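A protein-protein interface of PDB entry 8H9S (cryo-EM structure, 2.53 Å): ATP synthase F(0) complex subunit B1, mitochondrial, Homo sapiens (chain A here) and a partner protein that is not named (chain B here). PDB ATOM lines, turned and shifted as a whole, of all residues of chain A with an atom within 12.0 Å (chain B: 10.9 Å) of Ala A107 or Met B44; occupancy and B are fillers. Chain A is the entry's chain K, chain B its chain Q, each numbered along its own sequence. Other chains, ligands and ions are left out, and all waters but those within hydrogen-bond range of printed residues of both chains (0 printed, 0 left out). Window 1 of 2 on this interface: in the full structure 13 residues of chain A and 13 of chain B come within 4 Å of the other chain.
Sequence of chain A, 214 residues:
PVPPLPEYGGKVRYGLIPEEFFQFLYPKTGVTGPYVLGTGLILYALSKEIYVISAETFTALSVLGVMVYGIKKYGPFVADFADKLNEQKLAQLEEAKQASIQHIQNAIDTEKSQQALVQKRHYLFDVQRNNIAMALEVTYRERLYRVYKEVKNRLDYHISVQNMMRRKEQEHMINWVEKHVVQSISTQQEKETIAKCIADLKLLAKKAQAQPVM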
ATOM      1  N   GLN A  98      28.284 -15.926   3.169  1.00  0.00           N
ATOM      2  CA  GLN A  98      29.520 -15.731   3.918  1.00  0.00           C
ATOM      3  C   GLN A  98      29.436 -14.520   4.837  1.00  0.00           C
ATOM      4  O   GLN A  98      30.017 -14.529   5.928  1.00  0.00           O
ATOM      5  CB  GLN A  98      30.697 -15.585   2.959  1.00  0.00           C
ATOM      6  CG  GLN A  98      30.935 -16.804   2.095  1.00  0.00           C
ATOM      7  CD  GLN A  98      31.282 -18.028   2.909  1.00  0.00           C
ATOM      8  OE1 GLN A  98      30.784 -19.124   2.650  1.00  0.00           O
ATOM      9  NE2 GLN A  98      32.147 -17.852   3.899  1.00  0.00           N
ATOM     10  N   ALA A  99      28.714 -13.477   4.427  1.00  0.00           N
ATOM     11  CA  ALA A  99      28.607 -12.287   5.264  1.00  0.00           C
ATOM     12  C   ALA A  99      27.909 -12.591   6.582  1.00  0.00           C
ATOM     13  O   ALA A  99      28.347 -12.134   7.643  1.00  0.00           O
ATOM     14  CB  ALA A  99      27.872 -11.180   4.514  1.00  0.00           C
ATOM     15  N   SER A 100      26.828 -13.370   6.546  1.00  0.00           N
ATOM     16  CA  SER A 100      26.137 -13.673   7.793  1.00  0.00           C
ATOM     17  C   SER A 100      26.932 -14.652   8.642  1.00  0.00           C
ATOM     18  O   SER A 100      26.916 -14.557   9.878  1.00  0.00           O
ATOM     19  CB  SER A 100      24.743 -14.225   7.515  1.00  0.00           C
ATOM     20  OG  SER A 100      23.947 -14.173   8.686  1.00  0.00           O
ATOM     21  N   ILE A 101      27.635 -15.592   8.003  1.00  0.00           N
ATOM     22  CA  ILE A 101      28.553 -16.444   8.755  1.00  0.00           C
ATOM     23  C   ILE A 101      29.551 -15.588   9.527  1.00  0.00           C
ATOM     24  O   ILE A 101      29.772 -15.784  10.730  1.00  0.00           O
ATOM     25  CB  ILE A 101      29.267 -17.431   7.816  1.00  0.00           C
ATOM     26  CG1 ILE A 101      28.329 -18.570   7.433  1.00  0.00           C
ATOM     27  CG2 ILE A 101      30.512 -17.977   8.476  1.00  0.00           C
ATOM     28  CD1 ILE A 101      28.998 -19.655   6.638  1.00  0.00           C
ATOM     29  N   GLN A 102      30.159 -14.613   8.846  1.00  0.00           N
ATOM     30  CA  GLN A 102      31.132 -13.750   9.505  1.00  0.00           C
ATOM     31  C   GLN A 102      30.492 -12.936  10.618  1.00  0.00           C
ATOM     32  O   GLN A 102      31.110 -12.710  11.660  1.00  0.00           O
ATOM     33  CB  GLN A 102      31.796 -12.829   8.487  1.00  0.00           C
ATOM     34  CG  GLN A 102      33.079 -13.386   7.911  1.00  0.00           C
ATOM     35  CD  GLN A 102      34.128 -13.626   8.973  1.00  0.00           C
ATOM     36  OE1 GLN A 102      34.756 -12.688   9.461  1.00  0.00           O
ATOM     37  NE2 GLN A 102      34.323 -14.886   9.340  1.00  0.00           N
ATOM     38  N   HIS A 103      29.257 -12.479  10.415  1.00  0.00           N
ATOM     39  CA  HIS A 103      28.590 -11.703  11.456  1.00  0.00           C
ATOM     40  C   HIS A 103      28.415 -12.521  12.728  1.00  0.00           C
ATOM     41  O   HIS A 103      28.701 -12.045  13.836  1.00  0.00           O
ATOM     42  CB  HIS A 103      27.237 -11.206  10.968  1.00  0.00           C
ATOM     43  CG  HIS A 103      26.293 -10.867  12.077  1.00  0.00           C
ATOM     44  ND1 HIS A 103      26.246  -9.618  12.656  1.00  0.00           N
ATOM     45  CD2 HIS A 103      25.365 -11.615  12.720  1.00  0.00           C
ATOM     46  CE1 HIS A 103      25.327  -9.609  13.604  1.00  0.00           C
ATOM     47  NE2 HIS A 103      24.777 -10.809  13.664  1.00  0.00           N
ATOM     48  N   ILE A 104      27.932 -13.755  12.598  1.00  0.00           N
ATOM     49  CA  ILE A 104      27.703 -14.525  13.817  1.00  0.00           C
ATOM     50  C   ILE A 104      29.024 -14.969  14.436  1.00  0.00           C
ATOM     51  O   ILE A 104      29.130 -15.083  15.665  1.00  0.00           O
ATOM     52  CB  ILE A 104      26.753 -15.707  13.557  1.00  0.00           C
ATOM     53  CG1 ILE A 104      27.123 -16.421  12.264  1.00  0.00           C
ATOM     54  CG2 ILE A 104      25.316 -15.229  13.516  1.00  0.00           C
ATOM     55  CD1 ILE A 104      26.128 -17.457  11.845  1.00  0.00           C
ATOM     56  N   GLN A 105      30.061 -15.185  13.625  1.00  0.00           N
ATOM     57  CA  GLN A 105      31.368 -15.470  14.212  1.00  0.00           C
ATOM     58  C   GLN A 105      31.889 -14.272  14.996  1.00  0.00           C
ATOM     59  O   GLN A 105      32.473 -14.433  16.075  1.00  0.00           O
ATOM     60  CB  GLN A 105      32.359 -15.876  13.126  1.00  0.00           C
ATOM     61  CG  GLN A 105      33.732 -16.237  13.652  1.00  0.00           C
ATOM     62  CD  GLN A 105      33.803 -17.657  14.168  1.00  0.00           C
ATOM     63  OE1 GLN A 105      33.046 -18.048  15.053  1.00  0.00           O
ATOM     64  NE2 GLN A 105      34.717 -18.440  13.614  1.00  0.00           N
ATOM     65  N   ASN A 106      31.682 -13.063  14.475  1.00  0.00           N
ATOM     66  CA  ASN A 106      32.061 -11.864  15.210  1.00  0.00           C
ATOM     67  C   ASN A 106      31.302 -11.763  16.524  1.00  0.00           C
ATOM     68  O   ASN A 106      31.869 -11.368  17.547  1.00  0.00           O
ATOM     69  CB  ASN A 106      31.814 -10.623  14.360  1.00  0.00           C
ATOM     70  CG  ASN A 106      32.730 -10.550  13.171  1.00  0.00           C
ATOM     71  OD1 ASN A 106      33.563 -11.428  12.964  1.00  0.00           O
ATOM     72  ND2 ASN A 106      32.582  -9.501  12.373  1.00  0.00           N
ATOM     73  N   ALA A 107      30.012 -12.103  16.515  1.00  0.00           N
ATOM     74  CA  ALA A 107      29.245 -12.052  17.757  1.00  0.00           C
ATOM     75  C   ALA A 107      29.778 -13.052  18.778  1.00  0.00           C
ATOM     76  O   ALA A 107      29.878 -12.743  19.974  1.00  0.00           O
ATOM     77  CB  ALA A 107      27.769 -12.305  17.475  1.00  0.00           C
ATOM     78  N   ILE A 108      30.131 -14.256  18.324  1.00  0.00           N
ATOM     79  CA  ILE A 108      30.702 -15.257  19.226  1.00  0.00           C
ATOM     80  C   ILE A 108      32.011 -14.752  19.821  1.00  0.00           C
ATOM     81  O   ILE A 108      32.260 -14.877  21.030  1.00  0.00           O
ATOM     82  CB  ILE A 108      30.900 -16.592  18.487  1.00  0.00           C
ATOM     83  CG1 ILE A 108      29.590 -17.368  18.441  1.00  0.00           C
ATOM     84  CG2 ILE A 108      31.967 -17.422  19.157  1.00  0.00           C
ATOM     85  CD1 ILE A 108      29.677 -18.629  17.636  1.00  0.00           C
ATOM     86  N   ASP A 109      32.871 -14.184  18.975  1.00  0.00           N
ATOM     87  CA  ASP A 109      34.136 -13.639  19.455  1.00  0.00           C
ATOM     88  C   ASP A 109      33.905 -12.552  20.496  1.00  0.00           C
ATOM     89  O   ASP A 109      34.576 -12.514  21.536  1.00  0.00           O
ATOM     90  CB  ASP A 109      34.945 -13.094  18.282  1.00  0.00           C
ATOM     91  CG  ASP A 109      35.464 -14.187  17.379  1.00  0.00           C
ATOM     92  OD1 ASP A 109      35.299 -15.373  17.728  1.00  0.00           O
ATOM     93  OD2 ASP A 109      36.035 -13.861  16.319  1.00  0.00           O
ATOM     94  N   THR A 110      32.966 -11.647  20.222  1.00  0.00           N
ATOM     95  CA  THR A 110      32.656 -10.590  21.174  1.00  0.00           C
ATOM     96  C   THR A 110      32.219 -11.164  22.513  1.00  0.00           C
ATOM     97  O   THR A 110      32.655 -10.690  23.569  1.00  0.00           O
ATOM     98  CB  THR A 110      31.576  -9.675  20.601  1.00  0.00           C
ATOM     99  OG1 THR A 110      32.160  -8.795  19.634  1.00  0.00           O
ATOM    100  CG2 THR A 110      30.911  -8.864  21.696  1.00  0.00           C
ATOM    101  N   GLU A 111      31.373 -12.194  22.495  1.00  0.00           N
ATOM    102  CA  GLU A 111      30.904 -12.771  23.753  1.00  0.00           C
ATOM    103  C   GLU A 111      32.052 -13.408  24.530  1.00  0.00           C
ATOM    104  O   GLU A 111      32.150 -13.262  25.756  1.00  0.00           O
ATOM    105  CB  GLU A 111      29.799 -13.790  23.486  1.00  0.00           C
ATOM    106  CG  GLU A 111      28.462 -13.169  23.144  1.00  0.00           C
ATOM    107  CD  GLU A 111      27.796 -12.540  24.345  1.00  0.00           C
ATOM    108  OE1 GLU A 111      28.203 -12.857  25.479  1.00  0.00           O
ATOM    109  OE2 GLU A 111      26.863 -11.735  24.162  1.00  0.00           O
ATOM    110  N   LYS A 112      32.941 -14.114  23.830  1.00  0.00           N
ATOM    111  CA  LYS A 112      34.089 -14.702  24.515  1.00  0.00           C
ATOM    112  C   LYS A 112      34.999 -13.631  25.109  1.00  0.00           C
ATOM    113  O   LYS A 112      35.556 -13.818  26.199  1.00  0.00           O
ATOM    114  CB  LYS A 112      34.861 -15.602  23.558  1.00  0.00           C
ATOM    115  CG  LYS A 112      34.081 -16.833  23.131  1.00  0.00           C
ATOM    116  CD  LYS A 112      34.998 -17.908  22.575  1.00  0.00           C
ATOM    117  CE  LYS A 112      34.212 -19.141  22.188  1.00  0.00           C
ATOM    118  NZ  LYS A 112      33.041 -19.326  23.082  1.00  0.00           N
ATOM    119  N   SER A 113      35.145 -12.494  24.428  1.00  0.00           N
ATOM    120  CA  SER A 113      35.941 -11.406  24.990  1.00  0.00           C
ATOM    121  C   SER A 113      35.282 -10.820  26.234  1.00  0.00           C
ATOM    122  O   SER A 113      35.964 -10.493  27.217  1.00  0.00           O
ATOM    123  CB  SER A 113      36.167 -10.322  23.939  1.00  0.00           C
ATOM    124  OG  SER A 113      36.866 -10.848  22.827  1.00  0.00           O
ATOM    125  N   GLN A 114      33.960 -10.664  26.200  1.00  0.00           N
ATOM    126  CA  GLN A 114      33.240 -10.217  27.386  1.00  0.00           C
ATOM    127  C   GLN A 114      33.496 -11.162  28.553  1.00  0.00           C
ATOM    128  O   GLN A 114      33.675 -10.725  29.700  1.00  0.00           O
ATOM    129  CB  GLN A 114      31.748 -10.149  27.082  1.00  0.00           C
ATOM    130  CG  GLN A 114      31.377  -9.276  25.903  1.00  0.00           C
ATOM    131  CD  GLN A 114      31.559  -7.805  26.157  1.00  0.00           C
ATOM    132  OE1 GLN A 114      32.540  -7.207  25.714  1.00  0.00           O
ATOM    133  NE2 GLN A 114      30.582  -7.188  26.816  1.00  0.00           N
ATOM    134  N   GLN A 115      33.539 -12.466  28.269  1.00  0.00           N
ATOM    135  CA  GLN A 115      33.818 -13.441  29.320  1.00  0.00           C
ATOM    136  C   GLN A 115      35.239 -13.295  29.850  1.00  0.00           C
ATOM    137  O   GLN A 115      35.477 -13.455  31.051  1.00  0.00           O
ATOM    138  CB  GLN A 115      33.577 -14.858  28.805  1.00  0.00           C
ATOM    139  CG  GLN A 115      32.111 -15.175  28.572  1.00  0.00           C
ATOM    140  CD  GLN A 115      31.896 -16.519  27.923  1.00  0.00           C
ATOM    141  OE1 GLN A 115      30.772 -16.891  27.601  1.00  0.00           O
ATOM    142  NE2 GLN A 115      32.976 -17.258  27.727  1.00  0.00           N
ATOM    143  N   ALA A 116      36.195 -12.985  28.973  1.00  0.00           N
ATOM    144  CA  ALA A 116      37.566 -12.750  29.428  1.00  0.00           C
ATOM    145  C   ALA A 116      37.645 -11.563  30.389  1.00  0.00           C
ATOM    146  O   ALA A 116      38.321 -11.628  31.426  1.00  0.00           O
ATOM    147  CB  ALA A 116      38.482 -12.525  28.226  1.00  0.00           C
ATOM    148  N   LYS B  40      23.109  -8.314   7.355  1.00  0.00           N
ATOM    149  CA  LYS B  40      23.631  -7.282   8.292  1.00  0.00           C
ATOM    150  C   LYS B  40      24.631  -7.917   9.264  1.00  0.00           C
ATOM    151  O   LYS B  40      24.199  -8.694  10.139  1.00  0.00           O
ATOM    152  CB  LYS B  40      22.477  -6.598   9.035  1.00  0.00           C
ATOM    153  CG  LYS B  40      21.555  -5.742   8.176  1.00  0.00           C
ATOM    154  CD  LYS B  40      20.418  -5.107   8.951  1.00  0.00           C
ATOM    155  CE  LYS B  40      19.511  -4.236   8.105  1.00  0.00           C
ATOM    156  NZ  LYS B  40      18.399  -3.652   8.890  1.00  0.00           N
ATOM    157  N   PRO B  41      25.944  -7.607   9.134  1.00  0.00           N
ATOM    158  CA  PRO B  41      26.942  -8.094  10.073  1.00  0.00           C
ATOM    159  C   PRO B  41      26.892  -7.179  11.299  1.00  0.00           C
ATOM    160  O   PRO B  41      27.644  -7.415  12.226  1.00  0.00           O
ATOM    161  CB  PRO B  41      28.262  -7.920   9.315  1.00  0.00           C
ATOM    162  CG  PRO B  41      28.021  -6.695   8.465  1.00  0.00           C
ATOM    163  CD  PRO B  41      26.555  -6.766   8.091  1.00  0.00           C
ATOM    164  N   MET B  42      26.037  -6.149  11.270  1.00  0.00           N
ATOM    165  CA  MET B  42      25.906  -5.350  12.478  1.00  0.00           C
ATOM    166  C   MET B  42      24.545  -5.629  13.099  1.00  0.00           C
ATOM    167  O   MET B  42      23.574  -4.918  12.821  1.00  0.00           O
ATOM    168  CB  MET B  42      26.069  -3.862  12.173  1.00  0.00           C
ATOM    169  CG  MET B  42      26.007  -2.942  13.392  1.00  0.00           C
ATOM    170  SD  MET B  42      27.205  -3.320  14.690  1.00  0.00           S
ATOM    171  CE  MET B  42      26.227  -4.310  15.821  1.00  0.00           C
ATOM    172  N   LYS B  43      24.474  -6.670  13.924  1.00  0.00           N
ATOM    173  CA  LYS B  43      23.277  -6.941  14.709  1.00  0.00           C
ATOM    174  C   LYS B  43      23.651  -7.646  16.005  1.00  0.00           C
ATOM    175  O   LYS B  43      23.795  -8.872  16.037  1.00  0.00           O
ATOM    176  CB  LYS B  43      22.281  -7.781  13.910  1.00  0.00           C
ATOM    177  CG  LYS B  43      20.966  -8.027  14.635  1.00  0.00           C
ATOM    178  CD  LYS B  43      20.361  -6.725  15.142  1.00  0.00           C
ATOM    179  CE  LYS B  43      19.609  -6.934  16.449  1.00  0.00           C
ATOM    180  NZ  LYS B  43      20.508  -7.390  17.545  1.00  0.00           N
ATOM    181  N   MET B  44      23.803  -6.876  17.087  1.00  0.00           N
ATOM    182  CA  MET B  44      24.210  -7.412  18.374  1.00  0.00           C
ATOM    183  C   MET B  44      23.549  -6.582  19.477  1.00  0.00           C
ATOM    184  O   MET B  44      24.040  -5.531  19.888  1.00  0.00           O
ATOM    185  CB  MET B  44      25.733  -7.416  18.519  1.00  0.00           C
ATOM    186  CG  MET B  44      26.241  -8.142  19.754  1.00  0.00           C
ATOM    187  SD  MET B  44      25.939  -9.917  19.684  1.00  0.00           S
ATOM    188  CE  MET B  44      25.992 -10.341  21.416  1.00  0.00           C
ATOM    189  N   LYS B  45      22.410  -7.064  19.971  1.00  0.00           N
ATOM    190  CA  LYS B  45      21.770  -6.434  21.117  1.00  0.00           C
ATOM    191  C   LYS B  45      22.542  -6.821  22.371  1.00  0.00           C
ATOM    192  O   LYS B  45      22.087  -7.647  23.169  1.00  0.00           O
ATOM    193  CB  LYS B  45      20.299  -6.849  21.221  1.00  0.00           C
ATOM    194  CG  LYS B  45      19.557  -6.250  22.410  1.00  0.00           C
ATOM    195  CD  LYS B  45      18.506  -7.203  22.951  1.00  0.00           C
ATOM    196  CE  LYS B  45      17.780  -6.592  24.137  1.00  0.00           C
ATOM    197  NZ  LYS B  45      17.460  -5.154  23.909  1.00  0.00           N
ATOM    198  N   ASN B  46      23.736  -6.257  22.530  1.00  0.00           N
ATOM    199  CA  ASN B  46      24.578  -6.595  23.667  1.00  0.00           C
ATOM    200  C   ASN B  46      24.375  -5.606  24.804  1.00  0.00           C
ATOM    201  O   ASN B  46      23.540  -4.701  24.715  1.00  0.00           O
ATOM    202  CB  ASN B  46      26.050  -6.632  23.253  1.00  0.00           C
ATOM    203  CG  ASN B  46      26.855  -7.621  24.068  1.00  0.00           C
ATOM    204  OD1 ASN B  46      26.334  -8.250  24.987  1.00  0.00           O
ATOM    205  ND2 ASN B  46      28.134  -7.762  23.739  1.00  0.00           N
ATOM    206  N   TYR B  47      25.137  -5.782  25.878  1.00  0.00           N
ATOM    207  CA  TYR B  47      25.126  -4.846  26.988  1.00  0.00           C
ATOM    208  C   TYR B  47      26.443  -4.991  27.730  1.00  0.00           C
ATOM    209  O   TYR B  47      27.063  -6.057  27.715  1.00  0.00           O
ATOM    210  CB  TYR B  47      23.930  -5.086  27.922  1.00  0.00           C
ATOM    211  CG  TYR B  47      24.057  -4.448  29.291  1.00  0.00           C
ATOM    212  CD1 TYR B  47      24.043  -5.225  30.439  1.00  0.00           C
ATOM    213  CD2 TYR B  47      24.177  -3.073  29.434  1.00  0.00           C
ATOM    214  CE1 TYR B  47      24.160  -4.655  31.688  1.00  0.00           C
ATOM    215  CE2 TYR B  47      24.297  -2.493  30.679  1.00  0.00           C
ATOM    216  CZ  TYR B  47      24.285  -3.288  31.804  1.00  0.00           C
ATOM    217  OH  TYR B  47      24.399  -2.714  33.050  1.00  0.00           O
ATOM    218  N   ASN B  48      26.866  -3.898  28.360  1.00  0.00           N
ATOM    219  CA  ASN B  48      28.063  -3.895  29.188  1.00  0.00           C
ATOM    220  C   ASN B  48      28.049  -5.062  30.166  1.00  0.00           C
ATOM    221  O   ASN B  48      26.990  -5.575  30.530  1.00  0.00           O
ATOM    222  CB  ASN B  48      28.162  -2.573  29.954  1.00  0.00           C
ATOM    223  CG  ASN B  48      29.293  -2.565  30.963  1.00  0.00           C
ATOM    224  OD1 ASN B  48      30.415  -2.979  30.664  1.00  0.00           O
ATOM    225  ND2 ASN B  48      28.999  -2.105  32.171  1.00  0.00           N
ATOM    226  N   LYS B  49      29.236  -5.483  30.573  1.00  0.00           N
ATOM    227  CA  LYS B  49      29.421  -6.563  31.530  1.00  0.00           C
ATOM    228  C   LYS B  49      28.662  -6.225  32.811  1.00  0.00           C
ATOM    229  O   LYS B  49      28.294  -5.060  33.011  1.00  0.00           O
ATOM    230  CB  LYS B  49      30.910  -6.762  31.796  1.00  0.00           C
ATOM    231  CG  LYS B  49      31.654  -7.476  30.707  1.00  0.00           C
ATOM    232  CD  LYS B  49      31.925  -6.523  29.550  1.00  0.00           C
ATOM    233  CE  LYS B  49      32.910  -5.420  29.930  1.00  0.00           C
ATOM    234  NZ  LYS B  49      33.230  -4.489  28.799  1.00  0.00           N
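ND1 of His A103 lies within hydrogen-bond range of O of Lys B40, at 3.4 Å. O of Pro B41 is in hydrogen-bond range of ND1 of His A103. The backbone carbonyl oxygen of Lys B43 lies close to a ring nitrogen (NE2) of His A103 (3.2 Å).
The side-chain hydroxyl (OG1) of Thr A110 sits at hydrogen-bond distance from the backbone carbonyl oxygen (O) of Asn A106 (3.3 Å).
His A103 touches Met B42 (ND1 to N, 3.7 Å). SD of Met B44 touches CB of Ala A107, 3.7 Å away. CG2 of Thr A110 touches ND2 of Asn B46, at 3.6 Å. Glu A111 touches Met B44 (OE2 to CE, 3.2 Å). Glu A111 touches Asn B46 (OE2 to OD1, 3.6 Å). Gln A114 touches Asn B46. Gln A114 touches Tyr B47 (NE2 to O, 3.8 Å). Lys B49 touches Gln A114 (CD to NE2, 3.1 Å).
His A103 touches just these residues of chain B: Lys B40, Pro B41, Met B42 and Lys B43. Asn A106 touches none of the printed residues of chain B. Of chain B, only Met B44 comes within 4 Å of Ala A107. No residue of chain B comes within 4 Å of Asp A109. Thr A110 touches just one residue of chain B: Asn B46. Glu A111 touches just these residues of chain B: Met B44 (3.2 Å) and Asn B46 (3.6 Å). Of the printed residues of chain B, Gln A114 touches Asn B46 (3.97 Å), Tyr B47 (3.8 Å) and Lys B49 (3.1 Å). Ala A116 touches none of the printed residues of chain B. Printed residues of chain A within 4 Å of Lys B40: His A103. Printed residues of chain A within 4 Å of Pro B41: His A103. Of chain A, only His A103 comes within 4 Å of Met B42. No residue of chain A comes within 4 Å of Lys B45. Asn B46 touches just these residues of chain A: Thr A110 (3.6 Å), Glu A111 (3.6 Å) and Gln A114 (3.97 Å). Printed residues of chain A within 4 Å of Tyr B47: Gln A114 (3.8 Å). Of the printed residues of chain A, Lys B49 touches Gln A114 (3.1 Å). The nearest printed residue of chain A that does not touch Pro B41 is Ala A99 (4.5 Å).
Of the 10 printed residues of chain B, 8 touch a printed residue of chain A. Printed residues of chain B that touch a printed residue of chain A: Lys B40, Pro B41, Met B42, Lys B43, Met B44, Asn B46, Tyr B47 and Lys B49. Hydrophobic or aromatic side chains of chain B within 4 Å of the printed part of chain A: Pro B41 and Met B44. Among the printed residues, 11 pairs touch across the chains. Among the printed residues, no Asp or Glu carboxylate lies within 4 Å of a Lys or Arg side-chain nitrogen of the other chain.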
